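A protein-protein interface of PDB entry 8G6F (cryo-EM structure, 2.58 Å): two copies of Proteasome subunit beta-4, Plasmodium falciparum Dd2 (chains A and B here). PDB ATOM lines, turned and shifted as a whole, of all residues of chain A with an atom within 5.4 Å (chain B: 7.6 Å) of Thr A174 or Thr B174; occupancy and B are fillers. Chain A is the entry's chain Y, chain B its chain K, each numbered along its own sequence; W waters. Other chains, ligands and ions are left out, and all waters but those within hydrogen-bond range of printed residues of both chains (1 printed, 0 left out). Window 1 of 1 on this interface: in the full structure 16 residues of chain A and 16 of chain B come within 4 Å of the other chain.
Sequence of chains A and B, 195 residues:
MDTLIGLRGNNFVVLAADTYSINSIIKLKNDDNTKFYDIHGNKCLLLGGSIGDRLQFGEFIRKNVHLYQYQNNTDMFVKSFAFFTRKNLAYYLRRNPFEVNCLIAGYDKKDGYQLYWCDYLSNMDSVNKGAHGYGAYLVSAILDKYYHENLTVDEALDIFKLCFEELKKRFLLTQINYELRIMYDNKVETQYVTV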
ATOM      1  N   TYR A  20      13.636  37.129 -15.364  1.00  0.00           N
ATOM      2  CA  TYR A  20      12.709  36.245 -14.673  1.00  0.00           C
ATOM      3  C   TYR A  20      11.414  36.978 -14.355  1.00  0.00           C
ATOM      4  O   TYR A  20      11.436  38.107 -13.858  1.00  0.00           O
ATOM      5  CB  TYR A  20      13.328  35.705 -13.386  1.00  0.00           C
ATOM      6  CG  TYR A  20      14.530  34.832 -13.622  1.00  0.00           C
ATOM      7  CD1 TYR A  20      14.517  33.856 -14.602  1.00  0.00           C
ATOM      8  CD2 TYR A  20      15.679  34.988 -12.872  1.00  0.00           C
ATOM      9  CE1 TYR A  20      15.609  33.063 -14.825  1.00  0.00           C
ATOM     10  CE2 TYR A  20      16.777  34.196 -13.089  1.00  0.00           C
ATOM     11  CZ  TYR A  20      16.737  33.235 -14.065  1.00  0.00           C
ATOM     12  OH  TYR A  20      17.835  32.441 -14.282  1.00  0.00           O
ATOM     13  N   LYS A  27       8.862  30.478 -11.268  1.00  0.00           N
ATOM     14  CA  LYS A  27       9.239  31.440 -12.295  1.00  0.00           C
ATOM     15  C   LYS A  27       8.278  31.281 -13.464  1.00  0.00           C
ATOM     16  O   LYS A  27       8.306  30.264 -14.162  1.00  0.00           O
ATOM     17  CB  LYS A  27      10.683  31.220 -12.736  1.00  0.00           C
ATOM     18  CG  LYS A  27      11.703  31.401 -11.631  1.00  0.00           C
ATOM     19  CD  LYS A  27      13.126  31.359 -12.153  1.00  0.00           C
ATOM     20  CE  LYS A  27      13.523  29.960 -12.585  1.00  0.00           C
ATOM     21  NZ  LYS A  27      14.855  29.923 -13.238  1.00  0.00           N
ATOM     22  N   LEU A 167      26.572  36.800  -9.535  1.00  0.00           N
ATOM     23  CA  LEU A 167      25.175  36.575  -9.184  1.00  0.00           C
ATOM     24  C   LEU A 167      24.787  35.110  -9.323  1.00  0.00           C
ATOM     25  O   LEU A 167      23.911  34.631  -8.598  1.00  0.00           O
ATOM     26  CB  LEU A 167      24.268  37.441 -10.052  1.00  0.00           C
ATOM     27  CG  LEU A 167      24.230  38.918  -9.680  1.00  0.00           C
ATOM     28  CD1 LEU A 167      23.566  39.721 -10.779  1.00  0.00           C
ATOM     29  CD2 LEU A 167      23.518  39.116  -8.363  1.00  0.00           C
ATOM     30  N   LYS A 168      25.402  34.395 -10.259  1.00  0.00           N
ATOM     31  CA  LYS A 168      25.136  32.967 -10.386  1.00  0.00           C
ATOM     32  C   LYS A 168      25.778  32.186  -9.246  1.00  0.00           C
ATOM     33  O   LYS A 168      25.194  31.223  -8.738  1.00  0.00           O
ATOM     34  CB  LYS A 168      25.642  32.475 -11.742  1.00  0.00           C
ATOM     35  CG  LYS A 168      25.616  30.974 -11.946  1.00  0.00           C
ATOM     36  CD  LYS A 168      26.510  30.577 -13.107  1.00  0.00           C
ATOM     37  CE  LYS A 168      26.216  29.168 -13.590  1.00  0.00           C
ATOM     38  NZ  LYS A 168      26.016  28.222 -12.464  1.00  0.00           N
ATOM     39  N   PHE A 171      24.902  34.597  -5.161  1.00  0.00           N
ATOM     40  CA  PHE A 171      23.584  35.107  -4.820  1.00  0.00           C
ATOM     41  C   PHE A 171      22.643  33.960  -4.477  1.00  0.00           C
ATOM     42  O   PHE A 171      22.678  32.901  -5.107  1.00  0.00           O
ATOM     43  CB  PHE A 171      23.021  35.927  -5.980  1.00  0.00           C
ATOM     44  CG  PHE A 171      21.809  36.745  -5.632  1.00  0.00           C
ATOM     45  CD1 PHE A 171      21.617  37.243  -4.359  1.00  0.00           C
ATOM     46  CD2 PHE A 171      20.863  37.023  -6.594  1.00  0.00           C
ATOM     47  CE1 PHE A 171      20.505  37.991  -4.057  1.00  0.00           C
ATOM     48  CE2 PHE A 171      19.753  37.772  -6.295  1.00  0.00           C
ATOM     49  CZ  PHE A 171      19.574  38.255  -5.027  1.00  0.00           C
ATOM     50  N   LEU A 172      21.798  34.181  -3.468  1.00  0.00           N
ATOM     51  CA  LEU A 172      20.836  33.165  -3.056  1.00  0.00           C
ATOM     52  C   LEU A 172      19.995  32.694  -4.233  1.00  0.00           C
ATOM     53  O   LEU A 172      19.807  31.491  -4.438  1.00  0.00           O
ATOM     54  CB  LEU A 172      19.941  33.726  -1.951  1.00  0.00           C
ATOM     55  CG  LEU A 172      18.751  32.875  -1.516  1.00  0.00           C
ATOM     56  CD1 LEU A 172      19.229  31.689  -0.712  1.00  0.00           C
ATOM     57  CD2 LEU A 172      17.773  33.708  -0.713  1.00  0.00           C
ATOM     58  N   LEU A 173      19.462  33.633  -5.007  1.00  0.00           N
ATOM     59  CA  LEU A 173      18.741  33.309  -6.230  1.00  0.00           C
ATOM     60  C   LEU A 173      19.762  33.125  -7.342  1.00  0.00           C
ATOM     61  O   LEU A 173      20.376  34.095  -7.793  1.00  0.00           O
ATOM     62  CB  LEU A 173      17.747  34.413  -6.575  1.00  0.00           C
ATOM     63  CG  LEU A 173      16.833  34.881  -5.443  1.00  0.00           C
ATOM     64  CD1 LEU A 173      16.436  36.324  -5.642  1.00  0.00           C
ATOM     65  CD2 LEU A 173      15.603  34.004  -5.364  1.00  0.00           C
ATOM     66  N   THR A 174      19.958  31.887  -7.781  1.00  0.00           N
ATOM     67  CA  THR A 174      20.930  31.633  -8.835  1.00  0.00           C
ATOM     68  C   THR A 174      20.392  32.164 -10.152  1.00  0.00           C
ATOM     69  O   THR A 174      19.670  31.462 -10.865  1.00  0.00           O
ATOM     70  CB  THR A 174      21.239  30.140  -8.941  1.00  0.00           C
ATOM     71  OG1 THR A 174      21.618  29.638  -7.656  1.00  0.00           O
ATOM     72  CG2 THR A 174      22.356  29.894  -9.930  1.00  0.00           C
ATOM     73  N   GLN A 175      20.735  33.403 -10.483  1.00  0.00           N
ATOM     74  CA  GLN A 175      20.219  34.056 -11.675  1.00  0.00           C
ATOM     75  C   GLN A 175      21.184  33.830 -12.829  1.00  0.00           C
ATOM     76  O   GLN A 175      22.362  34.184 -12.739  1.00  0.00           O
ATOM     77  CB  GLN A 175      20.016  35.546 -11.421  1.00  0.00           C
ATOM     78  CG  GLN A 175      18.889  35.842 -10.465  1.00  0.00           C
ATOM     79  CD  GLN A 175      18.797  37.302 -10.119  1.00  0.00           C
ATOM     80  OE1 GLN A 175      19.809  37.983  -9.998  1.00  0.00           O
ATOM     81  NE2 GLN A 175      17.581  37.794  -9.950  1.00  0.00           N
ATOM     82  N   ILE A 176      20.679  33.250 -13.914  1.00  0.00           N
ATOM     83  CA  ILE A 176      21.516  32.868 -15.043  1.00  0.00           C
ATOM     84  C   ILE A 176      21.104  33.529 -16.348  1.00  0.00           C
ATOM     85  O   ILE A 176      21.871  33.462 -17.316  1.00  0.00           O
ATOM     86  CB  ILE A 176      21.547  31.334 -15.220  1.00  0.00           C
ATOM     87  CG1 ILE A 176      20.131  30.775 -15.329  1.00  0.00           C
ATOM     88  CG2 ILE A 176      22.266  30.683 -14.056  1.00  0.00           C
ATOM     89  CD1 ILE A 176      20.084  29.348 -15.790  1.00  0.00           C
ATOM     90  N   TYR B  20      23.324  23.498  -1.202  1.00  0.00           N
ATOM     91  CA  TYR B  20      23.549  24.906  -0.905  1.00  0.00           C
ATOM     92  C   TYR B  20      23.541  25.140   0.597  1.00  0.00           C
ATOM     93  O   TYR B  20      22.658  24.651   1.307  1.00  0.00           O
ATOM     94  CB  TYR B  20      22.487  25.779  -1.571  1.00  0.00           C
ATOM     95  CG  TYR B  20      22.531  25.729  -3.072  1.00  0.00           C
ATOM     96  CD1 TYR B  20      23.730  25.841  -3.754  1.00  0.00           C
ATOM     97  CD2 TYR B  20      21.376  25.563  -3.811  1.00  0.00           C
ATOM     98  CE1 TYR B  20      23.775  25.792  -5.120  1.00  0.00           C
ATOM     99  CE2 TYR B  20      21.413  25.513  -5.180  1.00  0.00           C
ATOM    100  CZ  TYR B  20      22.614  25.629  -5.829  1.00  0.00           C
ATOM    101  OH  TYR B  20      22.653  25.582  -7.199  1.00  0.00           O
ATOM    102  N   LYS B  27      24.922  32.503  -0.837  1.00  0.00           N
ATOM    103  CA  LYS B  27      25.169  31.076  -0.675  1.00  0.00           C
ATOM    104  C   LYS B  27      26.588  30.896  -0.153  1.00  0.00           C
ATOM    105  O   LYS B  27      27.556  31.164  -0.867  1.00  0.00           O
ATOM    106  CB  LYS B  27      24.972  30.344  -1.999  1.00  0.00           C
ATOM    107  CG  LYS B  27      23.558  30.418  -2.532  1.00  0.00           C
ATOM    108  CD  LYS B  27      23.380  29.611  -3.799  1.00  0.00           C
ATOM    109  CE  LYS B  27      24.297  30.093  -4.904  1.00  0.00           C
ATOM    110  NZ  LYS B  27      23.851  29.623  -6.237  1.00  0.00           N
ATOM    111  N   ASN B  30      28.321  26.104  -2.447  1.00  0.00           N
ATOM    112  CA  ASN B  30      27.543  25.379  -3.439  1.00  0.00           C
ATOM    113  C   ASN B  30      27.660  23.873  -3.272  1.00  0.00           C
ATOM    114  O   ASN B  30      26.997  23.130  -4.001  1.00  0.00           O
ATOM    115  CB  ASN B  30      27.986  25.771  -4.851  1.00  0.00           C
ATOM    116  CG  ASN B  30      27.634  27.205  -5.201  1.00  0.00           C
ATOM    117  OD1 ASN B  30      26.463  27.574  -5.265  1.00  0.00           O
ATOM    118  ND2 ASN B  30      28.650  28.021  -5.436  1.00  0.00           N
ATOM    119  N   PHE B 164      15.222  17.403 -10.981  1.00  0.00           N
ATOM    120  CA  PHE B 164      16.240  18.448 -10.928  1.00  0.00           C
ATOM    121  C   PHE B 164      16.056  19.450 -12.055  1.00  0.00           C
ATOM    122  O   PHE B 164      16.234  20.656 -11.856  1.00  0.00           O
ATOM    123  CB  PHE B 164      17.635  17.830 -10.995  1.00  0.00           C
ATOM    124  CG  PHE B 164      17.937  16.879  -9.878  1.00  0.00           C
ATOM    125  CD1 PHE B 164      17.304  16.992  -8.656  1.00  0.00           C
ATOM    126  CD2 PHE B 164      18.866  15.872 -10.049  1.00  0.00           C
ATOM    127  CE1 PHE B 164      17.591  16.118  -7.636  1.00  0.00           C
ATOM    128  CE2 PHE B 164      19.150  14.997  -9.033  1.00  0.00           C
ATOM    129  CZ  PHE B 164      18.517  15.120  -7.826  1.00  0.00           C
ATOM    130  N   LEU B 167      13.275  21.709 -11.035  1.00  0.00           N
ATOM    131  CA  LEU B 167      13.687  22.667 -10.014  1.00  0.00           C
ATOM    132  C   LEU B 167      14.593  23.747 -10.585  1.00  0.00           C
ATOM    133  O   LEU B 167      14.622  24.866 -10.069  1.00  0.00           O
ATOM    134  CB  LEU B 167      14.390  21.947  -8.867  1.00  0.00           C
ATOM    135  CG  LEU B 167      13.473  21.152  -7.946  1.00  0.00           C
ATOM    136  CD1 LEU B 167      14.285  20.226  -7.064  1.00  0.00           C
ATOM    137  CD2 LEU B 167      12.624  22.085  -7.114  1.00  0.00           C
ATOM    138  N   LYS B 168      15.357  23.427 -11.626  1.00  0.00           N
ATOM    139  CA  LYS B 168      16.173  24.446 -12.275  1.00  0.00           C
ATOM    140  C   LYS B 168      15.312  25.380 -13.118  1.00  0.00           C
ATOM    141  O   LYS B 168      15.560  26.589 -13.164  1.00  0.00           O
ATOM    142  CB  LYS B 168      17.247  23.772 -13.128  1.00  0.00           C
ATOM    143  CG  LYS B 168      17.978  24.678 -14.100  1.00  0.00           C
ATOM    144  CD  LYS B 168      18.780  23.866 -15.099  1.00  0.00           C
ATOM    145  CE  LYS B 168      19.931  24.667 -15.682  1.00  0.00           C
ATOM    146  NZ  LYS B 168      19.519  26.044 -16.052  1.00  0.00           N
ATOM    147  N   LYS B 169      14.290  24.843 -13.779  1.00  0.00           N
ATOM    148  CA  LYS B 169      13.540  25.623 -14.755  1.00  0.00           C
ATOM    149  C   LYS B 169      12.460  26.477 -14.101  1.00  0.00           C
ATOM    150  O   LYS B 169      12.329  27.663 -14.412  1.00  0.00           O
ATOM    151  CB  LYS B 169      12.916  24.687 -15.788  1.00  0.00           C
ATOM    152  CG  LYS B 169      11.987  25.372 -16.768  1.00  0.00           C
ATOM    153  CD  LYS B 169      11.302  24.371 -17.667  1.00  0.00           C
ATOM    154  CE  LYS B 169      10.564  25.067 -18.790  1.00  0.00           C
ATOM    155  NZ  LYS B 169       9.792  26.236 -18.305  1.00  0.00           N
ATOM    156  N   ARG B 170      11.668  25.889 -13.206  1.00  0.00           N
ATOM    157  CA  ARG B 170      10.451  26.528 -12.734  1.00  0.00           C
ATOM    158  C   ARG B 170      10.518  27.010 -11.294  1.00  0.00           C
ATOM    159  O   ARG B 170       9.730  27.880 -10.922  1.00  0.00           O
ATOM    160  CB  ARG B 170       9.266  25.562 -12.880  1.00  0.00           C
ATOM    161  CG  ARG B 170       7.888  26.201 -12.821  1.00  0.00           C
ATOM    162  CD  ARG B 170       7.647  27.175 -13.953  1.00  0.00           C
ATOM    163  NE  ARG B 170       7.378  26.494 -15.210  1.00  0.00           N
ATOM    164  CZ  ARG B 170       6.955  27.099 -16.309  1.00  0.00           C
ATOM    165  NH1 ARG B 170       6.742  28.401 -16.342  1.00  0.00           N
ATOM    166  NH2 ARG B 170       6.741  26.378 -17.404  1.00  0.00           N
ATOM    167  N   PHE B 171      11.425  26.482 -10.483  1.00  0.00           N
ATOM    168  CA  PHE B 171      11.500  26.897  -9.091  1.00  0.00           C
ATOM    169  C   PHE B 171      12.130  28.279  -8.982  1.00  0.00           C
ATOM    170  O   PHE B 171      13.097  28.594  -9.677  1.00  0.00           O
ATOM    171  CB  PHE B 171      12.304  25.879  -8.286  1.00  0.00           C
ATOM    172  CG  PHE B 171      12.209  26.052  -6.798  1.00  0.00           C
ATOM    173  CD1 PHE B 171      11.070  26.550  -6.202  1.00  0.00           C
ATOM    174  CD2 PHE B 171      13.272  25.700  -5.991  1.00  0.00           C
ATOM    175  CE1 PHE B 171      10.997  26.699  -4.838  1.00  0.00           C
ATOM    176  CE2 PHE B 171      13.199  25.845  -4.630  1.00  0.00           C
ATOM    177  CZ  PHE B 171      12.063  26.346  -4.054  1.00  0.00           C
ATOM    178  N   LEU B 172      11.575  29.105  -8.091  1.00  0.00           N
ATOM    179  CA  LEU B 172      12.085  30.459  -7.901  1.00  0.00           C
ATOM    180  C   LEU B 172      13.582  30.449  -7.626  1.00  0.00           C
ATOM    181  O   LEU B 172      14.338  31.238  -8.201  1.00  0.00           O
ATOM    182  CB  LEU B 172      11.330  31.132  -6.754  1.00  0.00           C
ATOM    183  CG  LEU B 172      11.901  32.421  -6.164  1.00  0.00           C
ATOM    184  CD1 LEU B 172      11.476  33.603  -6.997  1.00  0.00           C
ATOM    185  CD2 LEU B 172      11.440  32.588  -4.731  1.00  0.00           C
ATOM    186  N   LEU B 173      14.025  29.573  -6.731  1.00  0.00           N
ATOM    187  CA  LEU B 173      15.447  29.373  -6.487  1.00  0.00           C
ATOM    188  C   LEU B 173      15.972  28.411  -7.541  1.00  0.00           C
ATOM    189  O   LEU B 173      15.627  27.227  -7.533  1.00  0.00           O
ATOM    190  CB  LEU B 173      15.679  28.825  -5.082  1.00  0.00           C
ATOM    191  CG  LEU B 173      14.970  29.556  -3.942  1.00  0.00           C
ATOM    192  CD1 LEU B 173      14.732  28.622  -2.780  1.00  0.00           C
ATOM    193  CD2 LEU B 173      15.781  30.753  -3.498  1.00  0.00           C
ATOM    194  N   THR B 174      16.793  28.911  -8.457  1.00  0.00           N
ATOM    195  CA  THR B 174      17.314  28.057  -9.514  1.00  0.00           C
ATOM    196  C   THR B 174      18.375  27.131  -8.940  1.00  0.00           C
ATOM    197  O   THR B 174      19.558  27.476  -8.906  1.00  0.00           O
ATOM    198  CB  THR B 174      17.891  28.892 -10.655  1.00  0.00           C
ATOM    199  OG1 THR B 174      16.909  29.830 -11.104  1.00  0.00           O
ATOM    200  CG2 THR B 174      18.306  28.005 -11.809  1.00  0.00           C
ATOM    201  N   GLN B 175      17.959  25.955  -8.483  1.00  0.00           N
ATOM    202  CA  GLN B 175      18.859  25.015  -7.835  1.00  0.00           C
ATOM    203  C   GLN B 175      19.457  24.088  -8.882  1.00  0.00           C
ATOM    204  O   GLN B 175      18.727  23.427  -9.624  1.00  0.00           O
ATOM    205  CB  GLN B 175      18.119  24.218  -6.766  1.00  0.00           C
ATOM    206  CG  GLN B 175      17.733  25.044  -5.565  1.00  0.00           C
ATOM    207  CD  GLN B 175      16.838  24.295  -4.617  1.00  0.00           C
ATOM    208  OE1 GLN B 175      16.028  23.474  -5.033  1.00  0.00           O
ATOM    209  NE2 GLN B 175      16.976  24.573  -3.331  1.00  0.00           N
ATOM    210  N   ILE B 176      20.785  24.033  -8.932  1.00  0.00           N
ATOM    211  CA  ILE B 176      21.487  23.273  -9.957  1.00  0.00           C
ATOM    212  C   ILE B 176      22.420  22.215  -9.391  1.00  0.00           C
ATOM    213  O   ILE B 176      22.860  21.344 -10.150  1.00  0.00           O
ATOM    214  CB  ILE B 176      22.268  24.207 -10.907  1.00  0.00           C
ATOM    215  CG1 ILE B 176      23.192  25.129 -10.115  1.00  0.00           C
ATOM    216  CG2 ILE B 176      21.310  25.036 -11.740  1.00  0.00           C
ATOM    217  CD1 ILE B 176      24.184  25.861 -10.970  1.00  0.00           C
ATOM    218  N   ASN B 177      22.727  22.237  -8.095  1.00  0.00           N
ATOM    219  CA  ASN B 177      23.699  21.326  -7.497  1.00  0.00           C
ATOM    220  C   ASN B 177      23.005  20.413  -6.498  1.00  0.00           C
ATOM    221  O   ASN B 177      22.452  20.888  -5.500  1.00  0.00           O
ATOM    222  CB  ASN B 177      24.818  22.104  -6.804  1.00  0.00           C
ATOM    223  CG  ASN B 177      25.645  22.912  -7.768  1.00  0.00           C
ATOM    224  OD1 ASN B 177      26.228  22.373  -8.704  1.00  0.00           O
ATOM    225  ND2 ASN B 177      25.704  24.216  -7.546  1.00  0.00           N
ATOM    226  N   TYR B 178      23.087  19.104  -6.729  1.00  0.00           N
ATOM    227  CA  TYR B 178      22.408  18.124  -5.901  1.00  0.00           C
ATOM    228  C   TYR B 178      23.354  17.001  -5.511  1.00  0.00           C
ATOM    229  O   TYR B 178      24.267  16.643  -6.257  1.00  0.00           O
ATOM    230  CB  TYR B 178      21.197  17.536  -6.625  1.00  0.00           C
ATOM    231  CG  TYR B 178      20.238  18.581  -7.118  1.00  0.00           C
ATOM    232  CD1 TYR B 178      19.204  19.031  -6.317  1.00  0.00           C
ATOM    233  CD2 TYR B 178      20.367  19.122  -8.383  1.00  0.00           C
ATOM    234  CE1 TYR B 178      18.330  19.987  -6.761  1.00  0.00           C
ATOM    235  CE2 TYR B 178      19.498  20.076  -8.834  1.00  0.00           C
ATOM    236  CZ  TYR B 178      18.480  20.505  -8.020  1.00  0.00           C
ATOM    237  OH  TYR B 178      17.606  21.462  -8.469  1.00  0.00           O
ATOM    238  N   VAL B 195      22.847  20.320 -12.953  1.00  0.00           N
ATOM    239  CA  VAL B 195      22.001  20.561 -14.114  1.00  0.00           C
ATOM    240  C   VAL B 195      22.100  22.026 -14.521  1.00  0.00           C
ATOM    241  O   VAL B 195      22.655  22.353 -15.569  1.00  0.00           O
ATOM    242  CB  VAL B 195      20.536  20.168 -13.839  1.00  0.00           C
ATOM    243  CG1 VAL B 195      20.423  18.676 -13.610  1.00  0.00           C
ATOM    244  CG2 VAL B 195      19.987  20.932 -12.649  1.00  0.00           C
HETATM  245  O   HOH W   1      10.241  29.581 -15.502  1.00  0.00           O
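The side-chain amino group of Lys B27 sits at hydrogen-bond distance from the backbone carbonyl oxygen of Lys A168, 3.3 Å away. The side-chain amino group (NZ) of Lys B27 sits at hydrogen-bond distance from the side-chain hydroxyl (OG1) of Thr A174, at 2.6 Å. The backbone carbonyl oxygen (O) of Lys B168 sits at hydrogen-bond distance from the side-chain amino group (NZ) of Lys A27 (3.4 Å). O of Arg B170 is in hydrogen-bond range of N of Lys A27 (2.8 Å). OG1 of Thr B174 is in hydrogen-bond range of NZ of Lys A27 (3.0 Å). O of Thr A174 sits close to OG1 of Thr B174, 3.2 Å away.
Of the printed residues of chain B, Thr A174 touches Lys B27 and Thr B174. Gln A175 touches none of the printed residues of chain B. Printed residues of chain B within 4 Å of Ile A176: Lys B168 (3.4 Å). Printed residues of chain A within 4 Å of Lys B169: Lys A27 (3.2 Å). Printed residues of chain A within 4 Å of Leu B173: Leu A173 (3.8 Å). Thr B174 touches just these residues of chain A: Lys A27 (3.0 Å) and Thr A174 (3.1 Å). The nearest residue of chain A that does not touch Thr B174 is Tyr A20 (4.2 Å).
Water W1 lies within hydrogen-bond range of the backbone carbonyl oxygen (O) of Lys A27 (2.5 Å) and the backbone carbonyl oxygen (O) of Lys B169 (3.0 Å).
Hydrophobic or aromatic side chains of chain A that line the printed part of chain B: Leu A173 and Ile A176. Printed residues of chain B that touch a printed residue of chain A: Lys B27, Lys B168, Lys B169, Arg B170, Phe B171, Leu B172, Leu B173, Thr B174 and Ile B176. Hydrophobic or aromatic side chains of chain B within 4 Å of the printed part of chain A: Leu B173 and Ile B176. Among the printed residues, no Asp or Glu carboxylate lies within 4 Å of a Lys or Arg side-chain nitrogen of the other chain.
Among the printed residues, pairs that only touch across the chains: Lys A27 with Lys B169, Lys A27 with Phe B171, Lys A27 with Leu B172, Lys A168 with Ile B176, Phe A171 with Lys B27, Leu A172 with Lys B27, Leu A173 with Leu B173 and Ile A176 with Lys B168.
OH of Tyr B20 lies within hydrogen-bond range of N of Ile B176 (3.0 Å). NZ of Lys B27 lies close to OD1 of Asn B30 (3.5 Å). N of Val B195 lies within hydrogen-bond range of O of Ile B176 (3.0 Å). The side-chain hydroxyl (OH) of Tyr A20 is in hydrogen-bond range of the backbone NH (N) of Ile A176 (3.0 Å).
Lys A27 touches Phe B171, and with the chains exchanged Phe A171 touches Lys B27. Lys A27 touches Thr B174, and with the chains exchanged Thr A174 touches Lys B27. Lys A168 touches Ile B176, and with the chains exchanged Ile A176 touches Lys B168. Leu A173 touches its own counterpart, Leu B173. Positions printed for both chains: 20, 27, 167, 168, 171, 172, 173, 174, 175 and 176. Of the 14 pairs that touch across the chains among the printed residues, 12 have their exchanged pair printed and touching as well.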
